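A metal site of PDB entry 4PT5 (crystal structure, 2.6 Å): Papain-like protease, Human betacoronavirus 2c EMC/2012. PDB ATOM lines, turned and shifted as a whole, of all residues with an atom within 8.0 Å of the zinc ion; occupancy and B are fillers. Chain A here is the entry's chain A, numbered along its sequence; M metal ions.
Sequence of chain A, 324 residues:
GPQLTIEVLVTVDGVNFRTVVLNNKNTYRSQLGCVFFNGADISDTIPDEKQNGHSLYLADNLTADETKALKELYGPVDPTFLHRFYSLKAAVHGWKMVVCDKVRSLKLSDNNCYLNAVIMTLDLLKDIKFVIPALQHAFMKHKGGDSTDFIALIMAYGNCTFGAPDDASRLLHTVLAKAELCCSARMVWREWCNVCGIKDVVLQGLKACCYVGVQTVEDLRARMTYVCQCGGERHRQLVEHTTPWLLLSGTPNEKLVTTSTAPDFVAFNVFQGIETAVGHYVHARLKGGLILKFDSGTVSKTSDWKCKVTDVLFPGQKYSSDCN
The side-chain sulfur (SG) of Cys 230 lies close to the backbone NH (N) of Gly 232, 3.4 Å away.
SG of Cys 193 sits close to N of Val 195, 3.5 Å away.
SG of Cys 193 sits close to O of Glu 233 (3.6 Å).
Four residues have an atom within 4 Å of the zinc ion: Cys 193, Cys 196, Cys 228 and Cys 230.
The nearest printed residue that does not touch the zinc ion is Val 195 (4.4 Å).
The zinc ion is bound by the side-chain sulfur of Cys 230 (2.2 Å), the side-chain sulfur of Cys 193 (2.3 Å), the side-chain sulfur of Cys 228 (2.3 Å) and the side-chain sulfur of Cys 196 (2.3 Å).
The zinc ion has four donor atoms within binding distance.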
ATOM      1  N   TRP A 192     -10.165 -17.366 -23.578  1.00  0.00           N
ATOM      2  CA  TRP A 192     -10.592 -16.372 -24.565  1.00  0.00           C
ATOM      3  C   TRP A 192     -11.419 -15.235 -24.018  1.00  0.00           C
ATOM      4  O   TRP A 192     -12.002 -15.329 -22.941  1.00  0.00           O
ATOM      5  CB  TRP A 192     -11.320 -17.048 -25.729  1.00  0.00           C
ATOM      6  CG  TRP A 192     -12.785 -17.371 -25.485  1.00  0.00           C
ATOM      7  CD1 TRP A 192     -13.883 -16.603 -25.846  1.00  0.00           C
ATOM      8  CD2 TRP A 192     -13.340 -18.551 -24.818  1.00  0.00           C
ATOM      9  NE1 TRP A 192     -15.054 -17.212 -25.450  1.00  0.00           N
ATOM     10  CE2 TRP A 192     -14.805 -18.382 -24.830  1.00  0.00           C
ATOM     11  CE3 TRP A 192     -12.808 -19.692 -24.226  1.00  0.00           C
ATOM     12  CZ2 TRP A 192     -15.662 -19.318 -24.275  1.00  0.00           C
ATOM     13  CZ3 TRP A 192     -13.687 -20.630 -23.670  1.00  0.00           C
ATOM     14  CH2 TRP A 192     -15.082 -20.450 -23.694  1.00  0.00           C
ATOM     15  N   CYS A 193     -11.437 -14.155 -24.793  1.00  0.00           N
ATOM     16  CA  CYS A 193     -12.353 -13.032 -24.594  1.00  0.00           C
ATOM     17  C   CYS A 193     -12.918 -12.661 -25.967  1.00  0.00           C
ATOM     18  O   CYS A 193     -12.186 -12.645 -26.959  1.00  0.00           O
ATOM     19  CB  CYS A 193     -11.623 -11.842 -23.973  1.00  0.00           C
ATOM     20  SG  CYS A 193     -12.599 -10.312 -23.890  1.00  0.00           S
ATOM     21  N   ASN A 194     -14.218 -12.372 -26.007  1.00  0.00           N
ATOM     22  CA  ASN A 194     -14.902 -12.015 -27.255  1.00  0.00           C
ATOM     23  C   ASN A 194     -14.302 -10.806 -27.973  1.00  0.00           C
ATOM     24  O   ASN A 194     -14.420 -10.673 -29.192  1.00  0.00           O
ATOM     25  CB  ASN A 194     -16.394 -11.792 -27.002  1.00  0.00           C
ATOM     26  CG  ASN A 194     -17.087 -13.036 -26.471  1.00  0.00           C
ATOM     27  OD1 ASN A 194     -18.022 -12.933 -25.665  1.00  0.00           O
ATOM     28  ND2 ASN A 194     -16.644 -14.212 -26.911  1.00  0.00           N
ATOM     29  N   VAL A 195     -13.667  -9.924 -27.204  1.00  0.00           N
ATOM     30  CA  VAL A 195     -13.003  -8.734 -27.742  1.00  0.00           C
ATOM     31  C   VAL A 195     -11.499  -8.954 -27.920  1.00  0.00           C
ATOM     32  O   VAL A 195     -10.966  -8.749 -29.008  1.00  0.00           O
ATOM     33  CB  VAL A 195     -13.238  -7.484 -26.850  1.00  0.00           C
ATOM     34  CG1 VAL A 195     -12.719  -6.232 -27.533  1.00  0.00           C
ATOM     35  CG2 VAL A 195     -14.717  -7.336 -26.502  1.00  0.00           C
ATOM     36  N   CYS A 196     -10.828  -9.382 -26.847  1.00  0.00           N
ATOM     37  CA  CYS A 196      -9.363  -9.506 -26.810  1.00  0.00           C
ATOM     38  C   CYS A 196      -8.775 -10.615 -27.688  1.00  0.00           C
ATOM     39  O   CYS A 196      -7.635 -10.506 -28.136  1.00  0.00           O
ATOM     40  CB  CYS A 196      -8.873  -9.655 -25.367  1.00  0.00           C
ATOM     41  SG  CYS A 196      -9.221  -8.213 -24.341  1.00  0.00           S
ATOM     42  N   GLY A 197      -9.550 -11.676 -27.904  1.00  0.00           N
ATOM     43  CA  GLY A 197      -9.120 -12.776 -28.768  1.00  0.00           C
ATOM     44  C   GLY A 197      -9.026 -14.134 -28.092  1.00  0.00           C
ATOM     45  O   GLY A 197      -9.498 -14.310 -26.969  1.00  0.00           O
ATOM     46  N   VAL A 227     -13.438 -11.716 -14.799  1.00  0.00           N
ATOM     47  CA  VAL A 227     -13.291 -10.395 -15.429  1.00  0.00           C
ATOM     48  C   VAL A 227     -12.023 -10.297 -16.301  1.00  0.00           C
ATOM     49  O   VAL A 227     -10.952 -10.755 -15.902  1.00  0.00           O
ATOM     50  CB  VAL A 227     -13.306  -9.258 -14.364  1.00  0.00           C
ATOM     51  CG1 VAL A 227     -12.898  -7.924 -14.968  1.00  0.00           C
ATOM     52  CG2 VAL A 227     -14.682  -9.152 -13.724  1.00  0.00           C
ATOM     53  N   CYS A 228     -12.179  -9.698 -17.485  1.00  0.00           N
ATOM     54  CA  CYS A 228     -11.076  -9.528 -18.429  1.00  0.00           C
ATOM     55  C   CYS A 228     -10.281  -8.236 -18.212  1.00  0.00           C
ATOM     56  O   CYS A 228     -10.731  -7.321 -17.527  1.00  0.00           O
ATOM     57  CB  CYS A 228     -11.601  -9.571 -19.866  1.00  0.00           C
ATOM     58  SG  CYS A 228     -10.314  -9.504 -21.135  1.00  0.00           S
ATOM     59  N   GLN A 229      -9.088  -8.197 -18.807  1.00  0.00           N
ATOM     60  CA  GLN A 229      -8.248  -6.995 -18.870  1.00  0.00           C
ATOM     61  C   GLN A 229      -8.986  -5.808 -19.491  1.00  0.00           C
ATOM     62  O   GLN A 229      -8.838  -4.672 -19.034  1.00  0.00           O
ATOM     63  CB  GLN A 229      -6.961  -7.311 -19.657  1.00  0.00           C
ATOM     64  CG  GLN A 229      -5.974  -6.163 -19.809  1.00  0.00           C
ATOM     65  CD  GLN A 229      -6.214  -5.309 -21.053  1.00  0.00           C
ATOM     66  OE1 GLN A 229      -6.954  -5.690 -21.962  1.00  0.00           O
ATOM     67  NE2 GLN A 229      -5.567  -4.144 -21.097  1.00  0.00           N
ATOM     68  N   CYS A 230      -9.781  -6.079 -20.526  1.00  0.00           N
ATOM     69  CA  CYS A 230     -10.528  -5.032 -21.250  1.00  0.00           C
ATOM     70  C   CYS A 230     -11.743  -4.506 -20.480  1.00  0.00           C
ATOM     71  O   CYS A 230     -12.352  -3.523 -20.894  1.00  0.00           O
ATOM     72  CB  CYS A 230     -10.976  -5.554 -22.609  1.00  0.00           C
ATOM     73  SG  CYS A 230     -12.243  -6.838 -22.539  1.00  0.00           S
ATOM     74  N   GLY A 231     -12.082  -5.179 -19.385  1.00  0.00           N
ATOM     75  CA  GLY A 231     -13.256  -4.823 -18.582  1.00  0.00           C
ATOM     76  C   GLY A 231     -14.456  -5.688 -18.899  1.00  0.00           C
ATOM     77  O   GLY A 231     -15.505  -5.566 -18.260  1.00  0.00           O
ATOM     78  N   GLY A 232     -14.314  -6.556 -19.906  1.00  0.00           N
ATOM     79  CA  GLY A 232     -15.384  -7.453 -20.323  1.00  0.00           C
ATOM     80  C   GLY A 232     -15.416  -8.736 -19.508  1.00  0.00           C
ATOM     81  O   GLY A 232     -15.490  -8.698 -18.274  1.00  0.00           O
ATOM     82  N   GLU A 233     -15.362  -9.870 -20.205  1.00  0.00           N
ATOM     83  CA  GLU A 233     -15.366 -11.180 -19.556  1.00  0.00           C
ATOM     84  C   GLU A 233     -14.387 -12.159 -20.204  1.00  0.00           C
ATOM     85  O   GLU A 233     -14.315 -12.250 -21.433  1.00  0.00           O
ATOM     86  CB  GLU A 233     -16.771 -11.777 -19.551  1.00  0.00           C
ATOM     87  CG  GLU A 233     -17.670 -11.274 -18.427  1.00  0.00           C
ATOM     88  CD  GLU A 233     -19.081 -11.846 -18.484  1.00  0.00           C
ATOM     89  OE1 GLU A 233     -19.603 -12.220 -17.421  1.00  0.00           O
ATOM     90  OE2 GLU A 233     -19.660 -11.918 -19.592  1.00  0.00           O
ATOM     91  N   ARG A 234     -13.624 -12.859 -19.367  1.00  0.00           N
ATOM     92  CA  ARG A 234     -12.718 -13.917 -19.821  1.00  0.00           C
ATOM     93  C   ARG A 234     -13.282 -15.292 -19.489  1.00  0.00           C
ATOM     94  O   ARG A 234     -13.908 -15.487 -18.438  1.00  0.00           O
ATOM     95  CB  ARG A 234     -11.334 -13.775 -19.194  1.00  0.00           C
ATOM     96  CG  ARG A 234     -10.364 -12.925 -20.010  1.00  0.00           C
ATOM     97  CD  ARG A 234      -8.937 -13.109 -19.555  1.00  0.00           C
ATOM     98  NE  ARG A 234      -8.300 -14.248 -20.217  1.00  0.00           N
ATOM     99  CZ  ARG A 234      -7.031 -14.630 -20.027  1.00  0.00           C
ATOM    100  NH1 ARG A 234      -6.237 -13.954 -19.196  1.00  0.00           N
ATOM    101  NH2 ARG A 234      -6.563 -15.677 -20.677  1.00  0.00           N
HETATM  102 ZN    ZN M   1     -11.145  -8.690 -23.131  1.00  0.00          ZN
